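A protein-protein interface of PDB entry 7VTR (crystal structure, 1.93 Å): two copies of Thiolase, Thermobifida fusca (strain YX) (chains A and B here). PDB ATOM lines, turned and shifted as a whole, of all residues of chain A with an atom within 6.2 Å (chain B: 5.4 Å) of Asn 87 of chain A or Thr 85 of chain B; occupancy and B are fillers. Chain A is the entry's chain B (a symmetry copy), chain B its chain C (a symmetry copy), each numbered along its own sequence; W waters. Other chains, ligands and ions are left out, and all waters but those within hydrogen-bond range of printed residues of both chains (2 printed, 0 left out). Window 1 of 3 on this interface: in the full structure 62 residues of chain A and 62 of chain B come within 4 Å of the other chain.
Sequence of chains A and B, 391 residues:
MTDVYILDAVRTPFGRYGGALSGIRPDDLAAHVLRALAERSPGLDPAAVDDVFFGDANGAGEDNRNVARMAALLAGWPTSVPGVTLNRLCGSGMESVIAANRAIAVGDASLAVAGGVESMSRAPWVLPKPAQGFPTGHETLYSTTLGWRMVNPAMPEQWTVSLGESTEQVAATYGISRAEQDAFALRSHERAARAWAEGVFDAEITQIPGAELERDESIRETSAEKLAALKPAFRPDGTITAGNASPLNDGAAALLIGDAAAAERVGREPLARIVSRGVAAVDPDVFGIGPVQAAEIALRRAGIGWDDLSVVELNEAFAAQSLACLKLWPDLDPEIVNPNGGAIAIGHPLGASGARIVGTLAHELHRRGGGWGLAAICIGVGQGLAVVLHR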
ATOM      1  N   PHE A  54     -26.417  27.145  24.818  1.00  0.00           N
ATOM      2  CA  PHE A  54     -25.932  26.557  26.045  1.00  0.00           C
ATOM      3  C   PHE A  54     -24.781  25.636  25.707  1.00  0.00           C
ATOM      4  O   PHE A  54     -24.904  24.772  24.827  1.00  0.00           O
ATOM      5  CB  PHE A  54     -27.032  25.792  26.790  1.00  0.00           C
ATOM      6  CG  PHE A  54     -27.586  26.559  27.933  1.00  0.00           C
ATOM      7  CD1 PHE A  54     -28.656  27.404  27.739  1.00  0.00           C
ATOM      8  CD2 PHE A  54     -27.016  26.474  29.191  1.00  0.00           C
ATOM      9  CE1 PHE A  54     -29.174  28.138  28.789  1.00  0.00           C
ATOM     10  CE2 PHE A  54     -27.536  27.212  30.251  1.00  0.00           C
ATOM     11  CZ  PHE A  54     -28.610  28.051  30.036  1.00  0.00           C
ATOM     12  N   GLY A  55     -23.658  25.866  26.371  1.00  0.00           N
ATOM     13  CA  GLY A  55     -22.591  24.900  26.351  1.00  0.00           C
ATOM     14  C   GLY A  55     -22.934  23.774  27.311  1.00  0.00           C
ATOM     15  O   GLY A  55     -23.511  23.984  28.376  1.00  0.00           O
ATOM     16  N   ASP A  56     -22.592  22.570  26.905  1.00  0.00           N
ATOM     17  CA  ASP A  56     -22.893  21.389  27.695  1.00  0.00           C
ATOM     18  C   ASP A  56     -21.958  20.314  27.169  1.00  0.00           C
ATOM     19  O   ASP A  56     -22.024  19.969  25.986  1.00  0.00           O
ATOM     20  CB  ASP A  56     -24.366  20.996  27.565  1.00  0.00           C
ATOM     21  CG  ASP A  56     -24.786  19.984  28.606  1.00  0.00           C
ATOM     22  OD1 ASP A  56     -23.965  19.101  28.943  1.00  0.00           O
ATOM     23  OD2 ASP A  56     -25.935  20.058  29.082  1.00  0.00           O
ATOM     24  N   ALA A  57     -21.036  19.876  28.019  1.00  0.00           N
ATOM     25  CA  ALA A  57     -20.027  18.910  27.633  1.00  0.00           C
ATOM     26  C   ALA A  57     -20.569  17.494  27.598  1.00  0.00           C
ATOM     27  O   ALA A  57     -19.877  16.597  27.126  1.00  0.00           O
ATOM     28  CB  ALA A  57     -18.835  18.983  28.585  1.00  0.00           C
ATOM     29  N   ASN A  58     -21.792  17.280  28.068  1.00  0.00           N
ATOM     30  CA  ASN A  58     -22.325  15.928  28.167  1.00  0.00           C
ATOM     31  C   ASN A  58     -23.619  15.837  27.387  1.00  0.00           C
ATOM     32  O   ASN A  58     -23.622  15.583  26.181  1.00  0.00           O
ATOM     33  CB  ASN A  58     -22.535  15.573  29.638  1.00  0.00           C
ATOM     34  CG  ASN A  58     -22.709  14.087  29.880  1.00  0.00           C
ATOM     35  OD1 ASN A  58     -22.992  13.309  28.965  1.00  0.00           O
ATOM     36  ND2 ASN A  58     -22.483  13.679  31.131  1.00  0.00           N
ATOM     37  N   THR A  85     -27.515  23.852  21.602  1.00  0.00           N
ATOM     38  CA  THR A  85     -26.579  23.367  22.579  1.00  0.00           C
ATOM     39  C   THR A  85     -25.268  23.106  21.868  1.00  0.00           C
ATOM     40  O   THR A  85     -25.247  22.611  20.742  1.00  0.00           O
ATOM     41  CB  THR A  85     -27.116  22.106  23.240  1.00  0.00           C
ATOM     42  OG1 THR A  85     -28.373  22.434  23.837  1.00  0.00           O
ATOM     43  CG2 THR A  85     -26.158  21.599  24.297  1.00  0.00           C
ATOM     44  N   LEU A  86     -24.190  23.468  22.511  1.00  0.00           N
ATOM     45  CA  LEU A  86     -22.890  23.386  21.893  1.00  0.00           C
ATOM     46  C   LEU A  86     -21.972  22.620  22.814  1.00  0.00           C
ATOM     47  O   LEU A  86     -22.041  22.744  24.031  1.00  0.00           O
ATOM     48  CB  LEU A  86     -22.321  24.776  21.593  1.00  0.00           C
ATOM     49  CG  LEU A  86     -23.292  25.698  20.843  1.00  0.00           C
ATOM     50  CD1 LEU A  86     -24.190  26.467  21.777  1.00  0.00           C
ATOM     51  CD2 LEU A  86     -22.469  26.643  19.981  1.00  0.00           C
ATOM     52  N   ASN A  87     -21.142  21.805  22.198  1.00  0.00           N
ATOM     53  CA  ASN A  87     -20.217  20.942  22.902  1.00  0.00           C
ATOM     54  C   ASN A  87     -18.849  21.283  22.349  1.00  0.00           C
ATOM     55  O   ASN A  87     -18.495  20.846  21.255  1.00  0.00           O
ATOM     56  CB  ASN A  87     -20.556  19.476  22.673  1.00  0.00           C
ATOM     57  CG  ASN A  87     -19.752  18.565  23.536  1.00  0.00           C
ATOM     58  OD1 ASN A  87     -18.646  18.911  23.952  1.00  0.00           O
ATOM     59  ND2 ASN A  87     -20.269  17.363  23.770  1.00  0.00           N
ATOM     60  N   ARG A  88     -18.091  22.080  23.086  1.00  0.00           N
ATOM     61  CA  ARG A  88     -16.663  22.003  22.854  1.00  0.00           C
ATOM     62  C   ARG A  88     -16.071  21.617  24.198  1.00  0.00           C
ATOM     63  O   ARG A  88     -15.279  22.356  24.785  1.00  0.00           O
ATOM     64  CB  ARG A  88     -16.096  23.304  22.258  1.00  0.00           C
ATOM     65  CG  ARG A  88     -14.769  23.070  21.589  1.00  0.00           C
ATOM     66  CD  ARG A  88     -14.012  24.361  21.257  1.00  0.00           C
ATOM     67  NE  ARG A  88     -14.704  25.238  20.321  1.00  0.00           N
ATOM     68  CZ  ARG A  88     -14.478  25.252  19.012  1.00  0.00           C
ATOM     69  NH1 ARG A  88     -13.650  24.390  18.446  1.00  0.00           N
ATOM     70  NH2 ARG A  88     -15.100  26.151  18.253  1.00  0.00           N
ATOM     71  N   LEU A  89     -16.479  20.432  24.664  1.00  0.00           N
ATOM     72  CA  LEU A  89     -16.207  19.883  25.982  1.00  0.00           C
ATOM     73  C   LEU A  89     -16.096  20.972  27.038  1.00  0.00           C
ATOM     74  O   LEU A  89     -17.044  21.732  27.269  1.00  0.00           O
ATOM     75  CB  LEU A  89     -14.919  19.050  25.973  1.00  0.00           C
ATOM     76  CG  LEU A  89     -15.043  17.677  25.347  1.00  0.00           C
ATOM     77  CD1 LEU A  89     -13.737  16.905  25.538  1.00  0.00           C
ATOM     78  CD2 LEU A  89     -16.229  16.946  25.958  1.00  0.00           C
ATOM     79  N   CYS A  90     -14.915  21.051  27.653  1.00  0.00           N
ATOM     80  CA  CYS A  90     -14.689  21.919  28.802  1.00  0.00           C
ATOM     81  C   CYS A  90     -14.930  23.379  28.480  1.00  0.00           C
ATOM     82  O   CYS A  90     -15.186  24.176  29.387  1.00  0.00           O
ATOM     83  CB  CYS A  90     -13.248  21.756  29.288  1.00  0.00           C
ATOM     84  SG  CYS A  90     -12.701  20.073  29.332  1.00  0.00           S
ATOM     85  N   SER A  92     -17.288  24.541  26.446  1.00  0.00           N
ATOM     86  CA  SER A  92     -18.576  24.702  25.789  1.00  0.00           C
ATOM     87  C   SER A  92     -19.264  25.978  26.231  1.00  0.00           C
ATOM     88  O   SER A  92     -19.948  26.619  25.432  1.00  0.00           O
ATOM     89  CB  SER A  92     -19.479  23.510  26.074  1.00  0.00           C
ATOM     90  OG  SER A  92     -18.833  22.301  25.785  1.00  0.00           O
ATOM     91  N   GLU A  95     -17.709  28.630  24.253  1.00  0.00           N
ATOM     92  CA  GLU A  95     -18.217  28.467  22.906  1.00  0.00           C
ATOM     93  C   GLU A  95     -19.611  29.060  22.784  1.00  0.00           C
ATOM     94  O   GLU A  95     -19.907  29.724  21.792  1.00  0.00           O
ATOM     95  CB  GLU A  95     -18.227  26.996  22.509  1.00  0.00           C
ATOM     96  CG  GLU A  95     -18.684  26.788  21.084  1.00  0.00           C
ATOM     97  CD  GLU A  95     -17.666  27.276  20.092  1.00  0.00           C
ATOM     98  OE1 GLU A  95     -16.489  27.441  20.484  1.00  0.00           O
ATOM     99  OE2 GLU A  95     -18.014  27.465  18.909  1.00  0.00           O
ATOM    100  N   VAL B  52     -13.961  23.124  12.977  1.00  0.00           N
ATOM    101  CA  VAL B  52     -14.813  22.066  12.456  1.00  0.00           C
ATOM    102  C   VAL B  52     -16.075  22.092  13.289  1.00  0.00           C
ATOM    103  O   VAL B  52     -16.015  21.951  14.517  1.00  0.00           O
ATOM    104  CB  VAL B  52     -14.130  20.692  12.517  1.00  0.00           C
ATOM    105  CG1 VAL B  52     -15.068  19.601  12.030  1.00  0.00           C
ATOM    106  CG2 VAL B  52     -12.874  20.701  11.658  1.00  0.00           C
ATOM    107  N   PHE B  54     -19.729  20.321  13.782  1.00  0.00           N
ATOM    108  CA  PHE B  54     -20.528  19.161  13.447  1.00  0.00           C
ATOM    109  C   PHE B  54     -21.825  19.239  14.204  1.00  0.00           C
ATOM    110  O   PHE B  54     -21.836  19.473  15.421  1.00  0.00           O
ATOM    111  CB  PHE B  54     -19.828  17.853  13.759  1.00  0.00           C
ATOM    112  CG  PHE B  54     -19.254  17.202  12.553  1.00  0.00           C
ATOM    113  CD1 PHE B  54     -20.010  16.319  11.769  1.00  0.00           C
ATOM    114  CD2 PHE B  54     -17.940  17.464  12.202  1.00  0.00           C
ATOM    115  CE1 PHE B  54     -19.455  15.731  10.643  1.00  0.00           C
ATOM    116  CE2 PHE B  54     -17.368  16.880  11.090  1.00  0.00           C
ATOM    117  CZ  PHE B  54     -18.125  16.008  10.295  1.00  0.00           C
ATOM    118  N   GLY B  55     -22.910  19.108  13.455  1.00  0.00           N
ATOM    119  CA  GLY B  55     -24.184  18.895  14.045  1.00  0.00           C
ATOM    120  C   GLY B  55     -24.306  17.438  14.429  1.00  0.00           C
ATOM    121  O   GLY B  55     -23.861  16.538  13.717  1.00  0.00           O
ATOM    122  N   ASP B  56     -24.896  17.223  15.589  1.00  0.00           N
ATOM    123  CA  ASP B  56     -25.078  15.877  16.100  1.00  0.00           C
ATOM    124  C   ASP B  56     -26.194  15.977  17.112  1.00  0.00           C
ATOM    125  O   ASP B  56     -26.040  16.663  18.123  1.00  0.00           O
ATOM    126  CB  ASP B  56     -23.800  15.345  16.727  1.00  0.00           C
ATOM    127  CG  ASP B  56     -23.846  13.853  16.926  1.00  0.00           C
ATOM    128  OD1 ASP B  56     -24.946  13.337  17.205  1.00  0.00           O
ATOM    129  OD2 ASP B  56     -22.799  13.196  16.805  1.00  0.00           O
ATOM    130  N   ARG B  65     -18.297  13.410  23.426  1.00  0.00           N
ATOM    131  CA  ARG B  65     -17.189  14.262  23.824  1.00  0.00           C
ATOM    132  C   ARG B  65     -16.643  15.052  22.645  1.00  0.00           C
ATOM    133  O   ARG B  65     -15.436  15.120  22.409  1.00  0.00           O
ATOM    134  CB  ARG B  65     -16.116  13.447  24.537  1.00  0.00           C
ATOM    135  CG  ARG B  65     -16.486  13.265  26.037  1.00  0.00           C
ATOM    136  CD  ARG B  65     -15.483  12.411  26.752  1.00  0.00           C
ATOM    137  NE  ARG B  65     -14.260  13.148  27.042  1.00  0.00           N
ATOM    138  CZ  ARG B  65     -13.130  12.938  26.378  1.00  0.00           C
ATOM    139  NH1 ARG B  65     -13.056  12.015  25.433  1.00  0.00           N
ATOM    140  NH2 ARG B  65     -12.062  13.681  26.649  1.00  0.00           N
ATOM    141  N   ASN B  66     -17.569  15.685  21.921  1.00  0.00           N
ATOM    142  CA  ASN B  66     -17.261  16.635  20.865  1.00  0.00           C
ATOM    143  C   ASN B  66     -16.778  15.915  19.612  1.00  0.00           C
ATOM    144  O   ASN B  66     -15.583  15.923  19.290  1.00  0.00           O
ATOM    145  CB  ASN B  66     -16.241  17.664  21.337  1.00  0.00           C
ATOM    146  CG  ASN B  66     -16.061  18.764  20.334  1.00  0.00           C
ATOM    147  OD1 ASN B  66     -16.715  18.775  19.296  1.00  0.00           O
ATOM    148  ND2 ASN B  66     -15.132  19.643  20.594  1.00  0.00           N
ATOM    149  N   VAL B  67     -17.724  15.312  18.894  1.00  0.00           N
ATOM    150  CA  VAL B  67     -17.412  14.498  17.729  1.00  0.00           C
ATOM    151  C   VAL B  67     -16.694  15.296  16.652  1.00  0.00           C
ATOM    152  O   VAL B  67     -15.873  14.741  15.920  1.00  0.00           O
ATOM    153  CB  VAL B  67     -18.692  13.858  17.181  1.00  0.00           C
ATOM    154  CG1 VAL B  67     -19.518  14.883  16.414  1.00  0.00           C
ATOM    155  CG2 VAL B  67     -18.322  12.719  16.235  1.00  0.00           C
ATOM    156  N   ALA B  68     -16.975  16.594  16.541  1.00  0.00           N
ATOM    157  CA  ALA B  68     -16.281  17.416  15.554  1.00  0.00           C
ATOM    158  C   ALA B  68     -14.781  17.337  15.752  1.00  0.00           C
ATOM    159  O   ALA B  68     -14.026  17.132  14.798  1.00  0.00           O
ATOM    160  CB  ALA B  68     -16.750  18.865  15.652  1.00  0.00           C
ATOM    161  N   ARG B  69     -14.331  17.520  16.997  1.00  0.00           N
ATOM    162  CA  ARG B  69     -12.911  17.405  17.319  1.00  0.00           C
ATOM    163  C   ARG B  69     -12.408  15.984  17.135  1.00  0.00           C
ATOM    164  O   ARG B  69     -11.344  15.751  16.550  1.00  0.00           O
ATOM    165  CB  ARG B  69     -12.686  17.848  18.759  1.00  0.00           C
ATOM    166  CG  ARG B  69     -11.243  17.719  19.223  1.00  0.00           C
ATOM    167  CD  ARG B  69     -10.241  18.494  18.417  1.00  0.00           C
ATOM    168  NE  ARG B  69      -8.956  18.468  19.102  1.00  0.00           N
ATOM    169  CZ  ARG B  69      -7.808  18.820  18.543  1.00  0.00           C
ATOM    170  NH1 ARG B  69      -7.755  19.260  17.291  1.00  0.00           N
ATOM    171  NH2 ARG B  69      -6.691  18.736  19.258  1.00  0.00           N
ATOM    172  N   GLY B  83     -12.598  21.668  16.910  1.00  0.00           N
ATOM    173  CA  GLY B  83     -13.864  21.110  16.530  1.00  0.00           C
ATOM    174  C   GLY B  83     -14.881  21.417  17.600  1.00  0.00           C
ATOM    175  O   GLY B  83     -14.567  21.425  18.800  1.00  0.00           O
ATOM    176  N   VAL B  84     -16.090  21.716  17.162  1.00  0.00           N
ATOM    177  CA  VAL B  84     -17.196  21.966  18.065  1.00  0.00           C
ATOM    178  C   VAL B  84     -18.408  21.227  17.542  1.00  0.00           C
ATOM    179  O   VAL B  84     -18.644  21.153  16.328  1.00  0.00           O
ATOM    180  CB  VAL B  84     -17.476  23.470  18.256  1.00  0.00           C
ATOM    181  CG1 VAL B  84     -17.784  24.127  16.914  1.00  0.00           C
ATOM    182  CG2 VAL B  84     -18.668  23.652  19.171  1.00  0.00           C
ATOM    183  N   THR B  85     -19.163  20.658  18.467  1.00  0.00           N
ATOM    184  CA  THR B  85     -20.324  19.873  18.119  1.00  0.00           C
ATOM    185  C   THR B  85     -21.554  20.634  18.554  1.00  0.00           C
ATOM    186  O   THR B  85     -21.615  21.150  19.673  1.00  0.00           O
ATOM    187  CB  THR B  85     -20.250  18.500  18.780  1.00  0.00           C
ATOM    188  OG1 THR B  85     -19.052  17.854  18.333  1.00  0.00           O
ATOM    189  CG2 THR B  85     -21.471  17.687  18.385  1.00  0.00           C
ATOM    190  N   LEU B  86     -22.521  20.726  17.673  1.00  0.00           N
ATOM    191  CA  LEU B  86     -23.701  21.505  17.958  1.00  0.00           C
ATOM    192  C   LEU B  86     -24.923  20.620  17.936  1.00  0.00           C
ATOM    193  O   LEU B  86     -25.030  19.688  17.141  1.00  0.00           O
ATOM    194  CB  LEU B  86     -23.880  22.659  16.985  1.00  0.00           C
ATOM    195  CG  LEU B  86     -22.603  23.490  16.785  1.00  0.00           C
ATOM    196  CD1 LEU B  86     -21.628  22.894  15.778  1.00  0.00           C
ATOM    197  CD2 LEU B  86     -23.024  24.867  16.357  1.00  0.00           C
ATOM    198  N   ASN B  87     -25.851  20.945  18.809  1.00  0.00           N
ATOM    199  CA  ASN B  87     -27.083  20.185  18.890  1.00  0.00           C
ATOM    200  C   ASN B  87     -28.235  21.170  18.753  1.00  0.00           C
ATOM    201  O   ASN B  87     -28.585  21.871  19.710  1.00  0.00           O
ATOM    202  CB  ASN B  87     -27.148  19.410  20.193  1.00  0.00           C
ATOM    203  CG  ASN B  87     -28.351  18.512  20.256  1.00  0.00           C
ATOM    204  OD1 ASN B  87     -29.333  18.727  19.540  1.00  0.00           O
ATOM    205  ND2 ASN B  87     -28.261  17.455  21.067  1.00  0.00           N
HETATM  206  O   HOH W   1     -20.232  14.716  25.104  1.00  0.00           O
HETATM  207  O   HOH W   2     -23.793  19.697  21.300  1.00  0.00           O
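N of Asp 56 of chain A is in hydrogen-bond range of O of Leu 86 of chain A (2.9 Å). O of Phe 54 of chain B lies within hydrogen-bond range of N of Leu 86 of chain B, at 2.7 Å. NE of Arg 88 of chain A lies within salt-bridge range of OE1 of Glu 95 of chain A, at 2.8 Å. The backbone NH (N) of Leu 89 of chain A lies within hydrogen-bond range of the side-chain hydroxyl (OG) of Ser 92 of chain A (3.2 Å). The backbone NH of Arg 88 of chain A sits at hydrogen-bond distance from the side-chain hydroxyl of Ser 92 of chain A (2.8 Å). ND2 of Asn 66 of chain B lies within hydrogen-bond range of O of Gly 83 of chain B, 2.6 Å away.
Printed residues of chain A that touch a printed residue of chain B: Thr 85, Leu 86, Asn 87, Arg 88, Leu 89 and Glu 95. Hydrophobic or aromatic side chains of chain A within 4 Å of the printed part of chain B: Leu 89. Along chain A the printed residues that touch a printed residue of chain B span positions 85 to 95. Of the 14 printed residues of chain B, 7 touch a printed residue of chain A. Hydrophobic or aromatic side chains of chain B that line the printed part of chain A: Val 84 and Leu 86. Among the printed residues, 11 pairs touch across the chains. Among the printed residues, no Asp or Glu carboxylate lies within 4 Å of a Lys or Arg side-chain nitrogen of the other chain.
Of chain B, only Asn 66, Val 84 and Thr 85 come within 4 Å of Asn 87 of chain A. Of the printed residues of chain B, Arg 88 of chain A touches Asn 66, Gly 83 and Val 84. Asp 56 of chain B touches none of the printed residues of chain A. Val 67 of chain B touches none of the printed residues of chain A. Of the printed residues of chain A, Val 84 of chain B touches Asn 87, Arg 88 and Glu 95. The nearest residue of chain B that does not touch Asn 87 of chain A is Arg 65 of chain B (4.4 Å).
N of Asn 87 of chain A lies within hydrogen-bond range of O of Thr 85 of chain B (2.7 Å). The guanidinium group (NH1) of Arg 88 of chain A lies within hydrogen-bond range of the backbone carbonyl oxygen (O) of Gly 83 of chain B, at 3.1 Å. O of Thr 85 of chain A sits at hydrogen-bond distance from N of Asn 87 of chain B (2.6 Å). OD1 of Asn 66 of chain B lies close to O of Asn 87 of chain A, at 3.4 Å.
Among the printed residues, merely in contact across the chains: Thr 85 of chain A with Leu 86 of chain B (3.4 Å), Leu 86 of chain A with Thr 85 of chain B (3.4 Å), Asn 87 of chain A with Val 84 of chain B (3.5 Å), Arg 88 of chain A with Asn 66 of chain B (3.6 Å), Arg 88 of chain A with Val 84 of chain B (3.6 Å), Leu 89 of chain A with Arg 65 of chain B (3.6 Å) and Glu 95 of chain A with Val 84 of chain B (3.7 Å).
Water W1 lies within hydrogen-bond range of O of Ala 57 of chain A (2.8 Å), N of Arg 65 of chain B (2.9 Å) and ND2 of Asn 87 of chain A (3.0 Å). Water W2 lies within hydrogen-bond range of O of Thr 85 of chain B (3.1 Å), O of Thr 85 of chain A (3.3 Å) and N of Asn 87 of chain B (3.5 Å).
Thr 85 of chain A touches Leu 86 of chain B, and with the chains exchanged Leu 86 of chain A touches Thr 85 of chain B. Thr 85 of chain A touches Asn 87 of chain B, and with the chains exchanged Asn 87 of chain A touches Thr 85 of chain B.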
